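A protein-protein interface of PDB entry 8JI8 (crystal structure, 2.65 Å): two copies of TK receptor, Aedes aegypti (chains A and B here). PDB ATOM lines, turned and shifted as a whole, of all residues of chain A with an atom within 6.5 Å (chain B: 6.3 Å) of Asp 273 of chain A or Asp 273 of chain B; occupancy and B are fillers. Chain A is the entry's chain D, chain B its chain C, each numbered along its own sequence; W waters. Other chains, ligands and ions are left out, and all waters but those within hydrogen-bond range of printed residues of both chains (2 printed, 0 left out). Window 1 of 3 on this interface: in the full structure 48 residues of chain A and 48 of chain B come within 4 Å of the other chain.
OD1 of Asp 273 of chain A is in salt-bridge range of NH2 of Arg 279 of chain B (3.7 Å). The backbone carbonyl oxygen of Ser 278 of chain A sits at hydrogen-bond distance from the side-chain hydroxyl of Ser 155 of chain B. The side-chain hydroxyl (OG) of Ser 278 of chain B is in hydrogen-bond range of the backbone carbonyl oxygen (O) of Ser 155 of chain A. OD1 of Asp 154 of chain B lies within salt-bridge range of NH1 of Arg 279 of chain A. The side-chain hydroxyl (OG) of Ser 155 of chain B sits at hydrogen-bond distance from the guanidinium group (NH1) of Arg 279 of chain A, 3.0 Å away. The side-chain carboxylate (OD1) of Asp 273 of chain A is in hydrogen-bond range of the side-chain hydroxyl (OG1) of Thr 280 of chain B (2.8 Å).
O of Lys 271 of chain B is in hydrogen-bond range of N of Ser 155 of chain B. The backbone carbonyl oxygen (O) of Arg 279 of chain A lies within hydrogen-bond range of the backbone NH (N) of Ser 274 of chain A. O of Leu 272 of chain A lies within hydrogen-bond range of OG1 of Thr 280 of chain A, at 3.1 Å. The backbone NH (N) of Ser 155 of chain A sits at hydrogen-bond distance from the backbone carbonyl oxygen (O) of Lys 271 of chain A (3.1 Å).
Ser 155 of chain A touches Ser 278 of chain B, and with the chains exchanged Ser 278 of chain A touches Ser 155 of chain B. Leu 272 of chain A touches Arg 279 of chain B, but with the chains exchanged Arg 279 of chain A does not touch Leu 272 of chain B (6.2 Å). Of the 13 pairs that touch across the chains among the printed residues, 8 have their exchanged pair printed and touching as well.
CA of Lys 271 of chain A touches NH2 of Arg 279 of chain B, 3.8 Å away. Arg 279 of chain B touches Leu 272 of chain A (NH2 to O, 3.6 Å). OD2 of Asp 273 of chain A touches OD1 of Asp 273 of chain B, 3.7 Å away. NE of Arg 279 of chain A touches CD of Lys 271 of chain B, 3.8 Å away. Arg 279 of chain B touches Thr 280 of chain A (NH2 to OG1, 3.7 Å). Thr 280 of chain A touches Thr 280 of chain B (CB to OG1, 3.4 Å).
Water W1 bridges the backbone NH of Lys 271 of chain A (2.8 Å) and the guanidinium group of Arg 279 of chain B (3.1 Å). Water W2 bridges the side-chain carboxylate of Asp 273 of chain B (3.1 Å) and the side-chain carboxylate of Asp 273 of chain A (3.4 Å).
Printed residues of chain B within 4 Å of Leu 272 of chain A: Arg 279. Asp 273 of chain A touches three residues of chain B. Of the printed residues of chain B, Arg 279 of chain A touches Asp 154 (3.1 Å), Ser 155 (3.0 Å) and Lys 271 (3.8 Å). Of the printed residues of chain A, Lys 271 of chain B touches Arg 279. Asp 273 of chain B touches one residue of chain A. Of the printed residues of chain A, Ser 278 of chain B touches Ser 155 (2.5 Å). Of the printed residues of chain A, Thr 280 of chain B touches Asp 273 and Thr 280. The nearest residue of chain B that does not touch Asp 273 of chain A is Ser 278 of chain B (4.3 Å). The nearest residue of chain A that does not touch Asp 273 of chain B is Ser 278 of chain A (5.7 Å). The nearest printed residue of chain B that does not touch Thr 280 of chain A is Trp 281 of chain B (5.8 Å).
Of the 18 printed residues of chain A, 7 touch a printed residue of chain B. Along chain A the printed residues that touch a printed residue of chain B span positions 155 to 280. Of the 17 printed residues of chain B, 7 touch a printed residue of chain A. Printed residues of chain B that touch a printed residue of chain A: Asp 154, Ser 155, Lys 271, Asp 273, Ser 278, Arg 279 and Thr 280. Among the printed residues, 13 pairs touch across the chains. Among the printed residues, Asp or Glu carboxylates within 4 Å of a Lys or Arg side-chain nitrogen of the other chain: Asp 273 of chain A with Arg 279 of chain B (3.7 Å) and Arg 279 of chain A with Asp 154 of chain B (3.1 Å).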
ATOM      1  N   TYR A 120      33.904  -8.797  -2.230  1.00  0.00           N
ATOM      2  CA  TYR A 120      35.234  -8.654  -2.807  1.00  0.00           C
ATOM      3  C   TYR A 120      35.934  -7.422  -2.248  1.00  0.00           C
ATOM      4  O   TYR A 120      37.107  -7.479  -1.887  1.00  0.00           O
ATOM      5  CB  TYR A 120      35.120  -8.508  -4.328  1.00  0.00           C
ATOM      6  CG  TYR A 120      34.725  -9.758  -5.115  1.00  0.00           C
ATOM      7  CD1 TYR A 120      35.287 -11.005  -4.848  1.00  0.00           C
ATOM      8  CD2 TYR A 120      33.819  -9.675  -6.162  1.00  0.00           C
ATOM      9  CE1 TYR A 120      34.929 -12.127  -5.572  1.00  0.00           C
ATOM     10  CE2 TYR A 120      33.461 -10.787  -6.897  1.00  0.00           C
ATOM     11  CZ  TYR A 120      34.021 -12.016  -6.609  1.00  0.00           C
ATOM     12  OH  TYR A 120      33.646 -13.104  -7.357  1.00  0.00           O
ATOM     13  N   PRO A 149      37.165 -19.080  -3.680  1.00  0.00           N
ATOM     14  CA  PRO A 149      37.574 -20.026  -4.702  1.00  0.00           C
ATOM     15  C   PRO A 149      37.056 -19.698  -6.110  1.00  0.00           C
ATOM     16  O   PRO A 149      37.591 -20.237  -7.079  1.00  0.00           O
ATOM     17  CB  PRO A 149      37.038 -21.367  -4.162  1.00  0.00           C
ATOM     18  CG  PRO A 149      35.986 -21.013  -3.135  1.00  0.00           C
ATOM     19  CD  PRO A 149      36.460 -19.706  -2.551  1.00  0.00           C
ATOM     20  N   ASP A 150      36.050 -18.816  -6.237  1.00  0.00           N
ATOM     21  CA  ASP A 150      35.385 -18.582  -7.517  1.00  0.00           C
ATOM     22  C   ASP A 150      36.243 -17.733  -8.444  1.00  0.00           C
ATOM     23  O   ASP A 150      35.947 -17.674  -9.634  1.00  0.00           O
ATOM     24  CB  ASP A 150      34.015 -17.914  -7.380  1.00  0.00           C
ATOM     25  CG  ASP A 150      33.968 -16.754  -6.407  1.00  0.00           C
ATOM     26  OD1 ASP A 150      34.458 -16.922  -5.275  1.00  0.00           O
ATOM     27  OD2 ASP A 150      33.391 -15.722  -6.758  1.00  0.00           O
ATOM     28  N   LYS A 151      37.284 -17.085  -7.892  1.00  0.00           N
ATOM     29  CA  LYS A 151      38.248 -16.327  -8.672  1.00  0.00           C
ATOM     30  C   LYS A 151      39.426 -17.207  -9.106  1.00  0.00           C
ATOM     31  O   LYS A 151      40.362 -16.673  -9.706  1.00  0.00           O
ATOM     32  CB  LYS A 151      38.804 -15.161  -7.847  1.00  0.00           C
ATOM     33  CG  LYS A 151      37.910 -13.938  -7.651  1.00  0.00           C
ATOM     34  CD  LYS A 151      38.414 -13.040  -6.521  1.00  0.00           C
ATOM     35  CE  LYS A 151      38.256 -11.552  -6.769  1.00  0.00           C
ATOM     36  NZ  LYS A 151      38.758 -10.737  -5.627  1.00  0.00           N
ATOM     37  N   VAL A 153      39.178 -21.235  -9.613  1.00  0.00           N
ATOM     38  CA  VAL A 153      38.983 -22.584 -10.107  1.00  0.00           C
ATOM     39  C   VAL A 153      37.845 -22.588 -11.116  1.00  0.00           C
ATOM     40  O   VAL A 153      36.883 -21.852 -10.983  1.00  0.00           O
ATOM     41  CB  VAL A 153      38.722 -23.616  -8.987  1.00  0.00           C
ATOM     42  CG1 VAL A 153      39.819 -23.626  -7.940  1.00  0.00           C
ATOM     43  CG2 VAL A 153      37.393 -23.394  -8.301  1.00  0.00           C
ATOM     44  N   ASP A 154      37.987 -23.475 -12.103  1.00  0.00           N
ATOM     45  CA  ASP A 154      36.940 -23.796 -13.051  1.00  0.00           C
ATOM     46  C   ASP A 154      35.619 -23.950 -12.309  1.00  0.00           C
ATOM     47  O   ASP A 154      35.532 -24.664 -11.299  1.00  0.00           O
ATOM     48  CB  ASP A 154      37.291 -25.073 -13.814  1.00  0.00           C
ATOM     49  CG  ASP A 154      36.245 -25.552 -14.799  1.00  0.00           C
ATOM     50  OD1 ASP A 154      35.166 -24.903 -14.930  1.00  0.00           O
ATOM     51  OD2 ASP A 154      36.522 -26.575 -15.430  1.00  0.00           O
ATOM     52  N   SER A 155      34.610 -23.272 -12.874  1.00  0.00           N
ATOM     53  CA  SER A 155      33.289 -23.167 -12.300  1.00  0.00           C
ATOM     54  C   SER A 155      32.588 -24.518 -12.330  1.00  0.00           C
ATOM     55  O   SER A 155      31.610 -24.708 -11.616  1.00  0.00           O
ATOM     56  CB  SER A 155      32.503 -22.157 -13.044  1.00  0.00           C
ATOM     57  OG  SER A 155      32.321 -22.611 -14.368  1.00  0.00           O
ATOM     58  N   PHE A 158      32.295 -26.266  -8.866  1.00  0.00           N
ATOM     59  CA  PHE A 158      31.489 -25.714  -7.788  1.00  0.00           C
ATOM     60  C   PHE A 158      30.319 -26.625  -7.443  1.00  0.00           C
ATOM     61  O   PHE A 158      30.062 -26.850  -6.266  1.00  0.00           O
ATOM     62  CB  PHE A 158      31.048 -24.287  -8.104  1.00  0.00           C
ATOM     63  CG  PHE A 158      32.071 -23.333  -7.573  1.00  0.00           C
ATOM     64  CD1 PHE A 158      32.154 -23.108  -6.209  1.00  0.00           C
ATOM     65  CD2 PHE A 158      33.043 -22.802  -8.406  1.00  0.00           C
ATOM     66  CE1 PHE A 158      33.141 -22.285  -5.699  1.00  0.00           C
ATOM     67  CE2 PHE A 158      34.035 -21.984  -7.892  1.00  0.00           C
ATOM     68  CZ  PHE A 158      34.082 -21.729  -6.541  1.00  0.00           C
ATOM     69  N   LYS A 271      36.675 -19.671 -18.092  1.00  0.00           N
ATOM     70  CA  LYS A 271      35.894 -20.720 -17.444  1.00  0.00           C
ATOM     71  C   LYS A 271      35.679 -20.449 -15.947  1.00  0.00           C
ATOM     72  O   LYS A 271      35.392 -21.388 -15.199  1.00  0.00           O
ATOM     73  CB  LYS A 271      36.570 -22.091 -17.572  1.00  0.00           C
ATOM     74  CG  LYS A 271      37.114 -22.450 -18.950  1.00  0.00           C
ATOM     75  CD  LYS A 271      36.068 -22.666 -20.010  1.00  0.00           C
ATOM     76  CE  LYS A 271      36.677 -23.163 -21.304  1.00  0.00           C
ATOM     77  NZ  LYS A 271      37.379 -22.072 -22.013  1.00  0.00           N
ATOM     78  N   LEU A 272      35.822 -19.179 -15.526  1.00  0.00           N
ATOM     79  CA  LEU A 272      35.522 -18.737 -14.175  1.00  0.00           C
ATOM     80  C   LEU A 272      34.120 -18.133 -14.101  1.00  0.00           C
ATOM     81  O   LEU A 272      33.703 -17.444 -15.025  1.00  0.00           O
ATOM     82  CB  LEU A 272      36.522 -17.648 -13.792  1.00  0.00           C
ATOM     83  CG  LEU A 272      37.985 -18.054 -13.693  1.00  0.00           C
ATOM     84  CD1 LEU A 272      38.771 -16.908 -13.086  1.00  0.00           C
ATOM     85  CD2 LEU A 272      38.174 -19.322 -12.877  1.00  0.00           C
ATOM     86  N   ASP A 273      33.430 -18.343 -12.969  1.00  0.00           N
ATOM     87  CA  ASP A 273      32.144 -17.720 -12.682  1.00  0.00           C
ATOM     88  C   ASP A 273      32.171 -17.181 -11.253  1.00  0.00           C
ATOM     89  O   ASP A 273      32.542 -17.886 -10.317  1.00  0.00           O
ATOM     90  CB  ASP A 273      30.977 -18.705 -12.850  1.00  0.00           C
ATOM     91  CG  ASP A 273      30.365 -18.816 -14.244  1.00  0.00           C
ATOM     92  OD1 ASP A 273      30.410 -17.824 -15.017  1.00  0.00           O
ATOM     93  OD2 ASP A 273      29.833 -19.904 -14.549  1.00  0.00           O
ATOM     94  N   SER A 274      31.754 -15.926 -11.102  1.00  0.00           N
ATOM     95  CA  SER A 274      31.717 -15.226  -9.827  1.00  0.00           C
ATOM     96  C   SER A 274      30.437 -15.571  -9.082  1.00  0.00           C
ATOM     97  O   SER A 274      29.359 -15.273  -9.577  1.00  0.00           O
ATOM     98  CB  SER A 274      31.812 -13.723 -10.051  1.00  0.00           C
ATOM     99  OG  SER A 274      31.490 -12.995  -8.880  1.00  0.00           O
ATOM    100  N   LEU A 275      30.563 -16.162  -7.886  1.00  0.00           N
ATOM    101  CA  LEU A 275      29.406 -16.502  -7.067  1.00  0.00           C
ATOM    102  C   LEU A 275      28.870 -15.279  -6.312  1.00  0.00           C
ATOM    103  O   LEU A 275      27.706 -15.247  -5.915  1.00  0.00           O
ATOM    104  CB  LEU A 275      29.818 -17.616  -6.109  1.00  0.00           C
ATOM    105  CG  LEU A 275      30.106 -18.953  -6.783  1.00  0.00           C
ATOM    106  CD1 LEU A 275      30.457 -19.999  -5.733  1.00  0.00           C
ATOM    107  CD2 LEU A 275      28.922 -19.421  -7.631  1.00  0.00           C
ATOM    108  N   VAL A 276      29.725 -14.268  -6.134  1.00  0.00           N
ATOM    109  CA  VAL A 276      29.337 -12.994  -5.552  1.00  0.00           C
ATOM    110  C   VAL A 276      28.438 -12.210  -6.513  1.00  0.00           C
ATOM    111  O   VAL A 276      27.447 -11.614  -6.082  1.00  0.00           O
ATOM    112  CB  VAL A 276      30.597 -12.188  -5.178  1.00  0.00           C
ATOM    113  CG1 VAL A 276      30.288 -10.743  -4.824  1.00  0.00           C
ATOM    114  CG2 VAL A 276      31.372 -12.866  -4.061  1.00  0.00           C
ATOM    115  N   SER A 278      27.168 -13.605  -9.512  1.00  0.00           N
ATOM    116  CA  SER A 278      26.403 -14.527 -10.356  1.00  0.00           C
ATOM    117  C   SER A 278      26.469 -14.113 -11.830  1.00  0.00           C
ATOM    118  O   SER A 278      25.461 -14.177 -12.523  1.00  0.00           O
ATOM    119  CB  SER A 278      24.959 -14.675  -9.897  1.00  0.00           C
ATOM    120  OG  SER A 278      24.857 -15.296  -8.618  1.00  0.00           O
ATOM    121  N   ARG A 279      27.664 -13.689 -12.271  1.00  0.00           N
ATOM    122  CA  ARG A 279      27.992 -13.323 -13.643  1.00  0.00           C
ATOM    123  C   ARG A 279      29.322 -13.997 -13.977  1.00  0.00           C
ATOM    124  O   ARG A 279      30.000 -14.474 -13.070  1.00  0.00           O
ATOM    125  CB  ARG A 279      28.145 -11.804 -13.799  1.00  0.00           C
ATOM    126  CG  ARG A 279      26.848 -11.006 -13.722  1.00  0.00           C
ATOM    127  CD  ARG A 279      26.071 -10.978 -15.041  1.00  0.00           C
ATOM    128  NE  ARG A 279      24.796 -10.251 -14.997  1.00  0.00           N
ATOM    129  CZ  ARG A 279      23.644 -10.719 -14.509  1.00  0.00           C
ATOM    130  NH1 ARG A 279      23.539 -11.977 -14.100  1.00  0.00           N
ATOM    131  NH2 ARG A 279      22.583  -9.924 -14.452  1.00  0.00           N
ATOM    132  N   THR A 280      29.684 -14.056 -15.268  1.00  0.00           N
ATOM    133  CA  THR A 280      30.991 -14.554 -15.668  1.00  0.00           C
ATOM    134  C   THR A 280      31.955 -13.399 -15.908  1.00  0.00           C
ATOM    135  O   THR A 280      31.555 -12.233 -15.978  1.00  0.00           O
ATOM    136  CB  THR A 280      30.987 -15.348 -16.974  1.00  0.00           C
ATOM    137  OG1 THR A 280      32.343 -15.740 -17.186  1.00  0.00           O
ATOM    138  CG2 THR A 280      30.531 -14.568 -18.188  1.00  0.00           C
ATOM    139  N   TRP A 281      33.242 -13.756 -15.994  1.00  0.00           N
ATOM    140  CA  TRP A 281      34.226 -12.942 -16.680  1.00  0.00           C
ATOM    141  C   TRP A 281      34.138 -13.316 -18.161  1.00  0.00           C
ATOM    142  O   TRP A 281      34.606 -14.377 -18.569  1.00  0.00           O
ATOM    143  CB  TRP A 281      35.635 -13.172 -16.108  1.00  0.00           C
ATOM    144  CG  TRP A 281      35.897 -12.636 -14.721  1.00  0.00           C
ATOM    145  CD1 TRP A 281      36.439 -11.423 -14.407  1.00  0.00           C
ATOM    146  CD2 TRP A 281      35.685 -13.303 -13.459  1.00  0.00           C
ATOM    147  NE1 TRP A 281      36.556 -11.277 -13.049  1.00  0.00           N
ATOM    148  CE2 TRP A 281      36.118 -12.419 -12.443  1.00  0.00           C
ATOM    149  CE3 TRP A 281      35.167 -14.546 -13.085  1.00  0.00           C
ATOM    150  CZ2 TRP A 281      36.048 -12.738 -11.092  1.00  0.00           C
ATOM    151  CZ3 TRP A 281      35.101 -14.862 -11.743  1.00  0.00           C
ATOM    152  CH2 TRP A 281      35.529 -13.971 -10.761  1.00  0.00           C
ATOM    153  N   TYR B 120      19.597 -32.834 -19.070  1.00  0.00           N
ATOM    154  CA  TYR B 120      18.791 -32.167 -20.086  1.00  0.00           C
ATOM    155  C   TYR B 120      18.341 -33.182 -21.130  1.00  0.00           C
ATOM    156  O   TYR B 120      17.180 -33.183 -21.529  1.00  0.00           O
ATOM    157  CB  TYR B 120      19.527 -31.016 -20.772  1.00  0.00           C
ATOM    158  CG  TYR B 120      19.925 -29.810 -19.920  1.00  0.00           C
ATOM    159  CD1 TYR B 120      18.998 -29.123 -19.137  1.00  0.00           C
ATOM    160  CD2 TYR B 120      21.226 -29.313 -19.951  1.00  0.00           C
ATOM    161  CE1 TYR B 120      19.363 -28.006 -18.400  1.00  0.00           C
ATOM    162  CE2 TYR B 120      21.605 -28.201 -19.210  1.00  0.00           C
ATOM    163  CZ  TYR B 120      20.673 -27.545 -18.433  1.00  0.00           C
ATOM    164  OH  TYR B 120      21.050 -26.450 -17.719  1.00  0.00           O
ATOM    165  N   ASP B 150      17.184 -22.731 -14.462  1.00  0.00           N
ATOM    166  CA  ASP B 150      18.382 -22.087 -14.985  1.00  0.00           C
ATOM    167  C   ASP B 150      18.295 -21.781 -16.479  1.00  0.00           C
ATOM    168  O   ASP B 150      19.143 -21.056 -16.994  1.00  0.00           O
ATOM    169  CB  ASP B 150      19.649 -22.903 -14.726  1.00  0.00           C
ATOM    170  CG  ASP B 150      19.534 -24.355 -15.133  1.00  0.00           C
ATOM    171  OD1 ASP B 150      19.017 -25.142 -14.287  1.00  0.00           O
ATOM    172  OD2 ASP B 150      19.917 -24.673 -16.294  1.00  0.00           O
ATOM    173  N   LYS B 151      17.299 -22.307 -17.197  1.00  0.00           N
ATOM    174  CA  LYS B 151      17.192 -21.963 -18.605  1.00  0.00           C
ATOM    175  C   LYS B 151      16.167 -20.848 -18.806  1.00  0.00           C
ATOM    176  O   LYS B 151      15.869 -20.521 -19.958  1.00  0.00           O
ATOM    177  CB  LYS B 151      16.823 -23.187 -19.440  1.00  0.00           C
ATOM    178  CG  LYS B 151      17.941 -24.184 -19.734  1.00  0.00           C
ATOM    179  CD  LYS B 151      17.414 -25.480 -20.352  1.00  0.00           C
ATOM    180  CE  LYS B 151      18.415 -26.177 -21.251  1.00  0.00           C
ATOM    181  NZ  LYS B 151      17.762 -27.181 -22.132  1.00  0.00           N
ATOM    182  N   VAL B 153      15.846 -18.096 -16.113  1.00  0.00           N
ATOM    183  CA  VAL B 153      15.945 -17.219 -14.959  1.00  0.00           C
ATOM    184  C   VAL B 153      17.312 -16.541 -14.930  1.00  0.00           C
ATOM    185  O   VAL B 153      18.316 -17.223 -15.075  1.00  0.00           O
ATOM    186  CB  VAL B 153      15.685 -18.080 -13.711  1.00  0.00           C
ATOM    187  CG1 VAL B 153      16.449 -17.600 -12.505  1.00  0.00           C
ATOM    188  CG2 VAL B 153      14.192 -18.197 -13.419  1.00  0.00           C
ATOM    189  N   ASP B 154      17.343 -15.213 -14.732  1.00  0.00           N
ATOM    190  CA  ASP B 154      18.580 -14.474 -14.494  1.00  0.00           C
ATOM    191  C   ASP B 154      19.415 -15.242 -13.472  1.00  0.00           C
ATOM    192  O   ASP B 154      18.910 -15.583 -12.409  1.00  0.00           O
ATOM    193  CB  ASP B 154      18.288 -13.048 -14.006  1.00  0.00           C
ATOM    194  CG  ASP B 154      19.485 -12.144 -13.704  1.00  0.00           C
ATOM    195  OD1 ASP B 154      20.607 -12.653 -13.483  1.00  0.00           O
ATOM    196  OD2 ASP B 154      19.287 -10.905 -13.679  1.00  0.00           O
ATOM    197  N   SER B 155      20.693 -15.487 -13.784  1.00  0.00           N
ATOM    198  CA  SER B 155      21.594 -16.236 -12.911  1.00  0.00           C
ATOM    199  C   SER B 155      21.665 -15.657 -11.493  1.00  0.00           C
ATOM    200  O   SER B 155      21.928 -16.405 -10.544  1.00  0.00           O
ATOM    201  CB  SER B 155      22.972 -16.313 -13.509  1.00  0.00           C
ATOM    202  OG  SER B 155      23.436 -15.009 -13.832  1.00  0.00           O
ATOM    203  N   PHE B 158      19.860 -17.321  -8.109  1.00  0.00           N
ATOM    204  CA  PHE B 158      20.147 -18.632  -7.549  1.00  0.00           C
ATOM    205  C   PHE B 158      20.809 -18.501  -6.184  1.00  0.00           C
ATOM    206  O   PHE B 158      20.513 -19.304  -5.302  1.00  0.00           O
ATOM    207  CB  PHE B 158      20.983 -19.491  -8.504  1.00  0.00           C
ATOM    208  CG  PHE B 158      20.169 -20.114  -9.607  1.00  0.00           C
ATOM    209  CD1 PHE B 158      19.231 -21.088  -9.313  1.00  0.00           C
ATOM    210  CD2 PHE B 158      20.271 -19.670 -10.912  1.00  0.00           C
ATOM    211  CE1 PHE B 158      18.433 -21.638 -10.297  1.00  0.00           C
ATOM    212  CE2 PHE B 158      19.474 -20.225 -11.904  1.00  0.00           C
ATOM    213  CZ  PHE B 158      18.549 -21.202 -11.593  1.00  0.00           C
ATOM    214  N   LYS B 271      22.682 -13.844 -19.910  1.00  0.00           N
ATOM    215  CA  LYS B 271      22.729 -13.758 -18.459  1.00  0.00           C
ATOM    216  C   LYS B 271      22.172 -15.033 -17.809  1.00  0.00           C
ATOM    217  O   LYS B 271      21.711 -14.952 -16.665  1.00  0.00           O
ATOM    218  CB  LYS B 271      21.897 -12.597 -17.881  1.00  0.00           C
ATOM    219  CG  LYS B 271      21.912 -11.254 -18.599  1.00  0.00           C
ATOM    220  CD  LYS B 271      23.169 -10.425 -18.373  1.00  0.00           C
ATOM    221  CE  LYS B 271      23.149  -9.081 -19.081  1.00  0.00           C
ATOM    222  NZ  LYS B 271      23.389  -9.206 -20.543  1.00  0.00           N
ATOM    223  N   LEU B 272      22.213 -16.192 -18.500  1.00  0.00           N
ATOM    224  CA  LEU B 272      21.824 -17.473 -17.896  1.00  0.00           C
ATOM    225  C   LEU B 272      23.047 -18.269 -17.420  1.00  0.00           C
ATOM    226  O   LEU B 272      24.083 -18.277 -18.082  1.00  0.00           O
ATOM    227  CB  LEU B 272      21.075 -18.330 -18.926  1.00  0.00           C
ATOM    228  CG  LEU B 272      19.801 -17.750 -19.526  1.00  0.00           C
ATOM    229  CD1 LEU B 272      19.281 -18.674 -20.614  1.00  0.00           C
ATOM    230  CD2 LEU B 272      18.740 -17.535 -18.459  1.00  0.00           C
ATOM    231  N   ASP B 273      22.893 -19.015 -16.318  1.00  0.00           N
ATOM    232  CA  ASP B 273      23.945 -19.888 -15.801  1.00  0.00           C
ATOM    233  C   ASP B 273      23.391 -21.307 -15.709  1.00  0.00           C
ATOM    234  O   ASP B 273      22.449 -21.543 -14.965  1.00  0.00           O
ATOM    235  CB  ASP B 273      24.467 -19.424 -14.427  1.00  0.00           C
ATOM    236  CG  ASP B 273      25.663 -20.184 -13.851  1.00  0.00           C
ATOM    237  OD1 ASP B 273      26.269 -21.010 -14.576  1.00  0.00           O
ATOM    238  OD2 ASP B 273      25.997 -19.948 -12.666  1.00  0.00           O
ATOM    239  N   SER B 274      23.990 -22.241 -16.453  1.00  0.00           N
ATOM    240  CA  SER B 274      23.565 -23.629 -16.402  1.00  0.00           C
ATOM    241  C   SER B 274      24.194 -24.352 -15.218  1.00  0.00           C
ATOM    242  O   SER B 274      25.339 -24.785 -15.302  1.00  0.00           O
ATOM    243  CB  SER B 274      23.901 -24.357 -17.654  1.00  0.00           C
ATOM    244  OG  SER B 274      23.520 -25.718 -17.522  1.00  0.00           O
ATOM    245  N   LEU B 275      23.395 -24.574 -14.168  1.00  0.00           N
ATOM    246  CA  LEU B 275      23.824 -25.348 -13.009  1.00  0.00           C
ATOM    247  C   LEU B 275      24.208 -26.781 -13.394  1.00  0.00           C
ATOM    248  O   LEU B 275      24.966 -27.432 -12.672  1.00  0.00           O
ATOM    249  CB  LEU B 275      22.688 -25.355 -11.979  1.00  0.00           C
ATOM    250  CG  LEU B 275      22.316 -23.996 -11.378  1.00  0.00           C
ATOM    251  CD1 LEU B 275      21.061 -24.102 -10.522  1.00  0.00           C
ATOM    252  CD2 LEU B 275      23.476 -23.426 -10.565  1.00  0.00           C
ATOM    253  N   VAL B 276      23.698 -27.258 -14.536  1.00  0.00           N
ATOM    254  CA  VAL B 276      23.924 -28.614 -14.989  1.00  0.00           C
ATOM    255  C   VAL B 276      25.313 -28.735 -15.611  1.00  0.00           C
ATOM    256  O   VAL B 276      26.038 -29.688 -15.339  1.00  0.00           O
ATOM    257  CB  VAL B 276      22.814 -29.017 -15.967  1.00  0.00           C
ATOM    258  CG1 VAL B 276      23.079 -30.359 -16.625  1.00  0.00           C
ATOM    259  CG2 VAL B 276      21.455 -28.999 -15.278  1.00  0.00           C
ATOM    260  N   SER B 278      27.431 -26.433 -14.956  1.00  0.00           N
ATOM    261  CA  SER B 278      28.129 -25.553 -14.024  1.00  0.00           C
ATOM    262  C   SER B 278      28.956 -24.503 -14.776  1.00  0.00           C
ATOM    263  O   SER B 278      30.070 -24.183 -14.362  1.00  0.00           O
ATOM    264  CB  SER B 278      28.951 -26.363 -13.032  1.00  0.00           C
ATOM    265  OG  SER B 278      29.279 -25.613 -11.864  1.00  0.00           O
ATOM    266  N   ARG B 279      28.368 -23.962 -15.862  1.00  0.00           N
ATOM    267  CA  ARG B 279      28.989 -22.987 -16.747  1.00  0.00           C
ATOM    268  C   ARG B 279      27.933 -22.070 -17.365  1.00  0.00           C
ATOM    269  O   ARG B 279      26.927 -22.539 -17.895  1.00  0.00           O
ATOM    270  CB  ARG B 279      29.743 -23.655 -17.904  1.00  0.00           C
ATOM    271  CG  ARG B 279      31.258 -23.627 -17.775  1.00  0.00           C
ATOM    272  CD  ARG B 279      31.873 -22.244 -17.591  1.00  0.00           C
ATOM    273  NE  ARG B 279      31.889 -21.421 -18.801  1.00  0.00           N
ATOM    274  CZ  ARG B 279      32.145 -20.114 -18.825  1.00  0.00           C
ATOM    275  NH1 ARG B 279      32.249 -19.476 -19.980  1.00  0.00           N
ATOM    276  NH2 ARG B 279      32.310 -19.452 -17.690  1.00  0.00           N
ATOM    277  N   THR B 280      28.230 -20.766 -17.365  1.00  0.00           N
ATOM    278  CA  THR B 280      27.396 -19.751 -17.991  1.00  0.00           C
ATOM    279  C   THR B 280      27.297 -19.983 -19.501  1.00  0.00           C
ATOM    280  O   THR B 280      28.114 -20.668 -20.100  1.00  0.00           O
ATOM    281  CB  THR B 280      27.875 -18.336 -17.608  1.00  0.00           C
ATOM    282  OG1 THR B 280      29.303 -18.291 -17.529  1.00  0.00           O
ATOM    283  CG2 THR B 280      27.316 -17.854 -16.284  1.00  0.00           C
ATOM    284  N   TRP B 281      26.230 -19.451 -20.100  1.00  0.00           N
ATOM    285  CA  TRP B 281      26.034 -19.530 -21.538  1.00  0.00           C
ATOM    286  C   TRP B 281      26.847 -18.427 -22.200  1.00  0.00           C
ATOM    287  O   TRP B 281      26.832 -17.293 -21.729  1.00  0.00           O
ATOM    288  CB  TRP B 281      24.567 -19.328 -21.918  1.00  0.00           C
ATOM    289  CG  TRP B 281      23.631 -20.420 -21.480  1.00  0.00           C
ATOM    290  CD1 TRP B 281      23.093 -20.676 -20.248  1.00  0.00           C
ATOM    291  CD2 TRP B 281      23.104 -21.422 -22.362  1.00  0.00           C
ATOM    292  NE1 TRP B 281      22.264 -21.766 -20.305  1.00  0.00           N
ATOM    293  CE2 TRP B 281      22.261 -22.249 -21.583  1.00  0.00           C
ATOM    294  CE3 TRP B 281      23.273 -21.674 -23.722  1.00  0.00           C
ATOM    295  CZ2 TRP B 281      21.593 -23.329 -22.129  1.00  0.00           C
ATOM    296  CZ3 TRP B 281      22.618 -22.757 -24.254  1.00  0.00           C
ATOM    297  CH2 TRP B 281      21.781 -23.558 -23.474  1.00  0.00           C
HETATM  298  O   HOH W   1      35.186 -18.620 -20.255  1.00  0.00           O
HETATM  299  O   HOH W   2      28.355 -21.922 -12.224  1.00  0.00           O
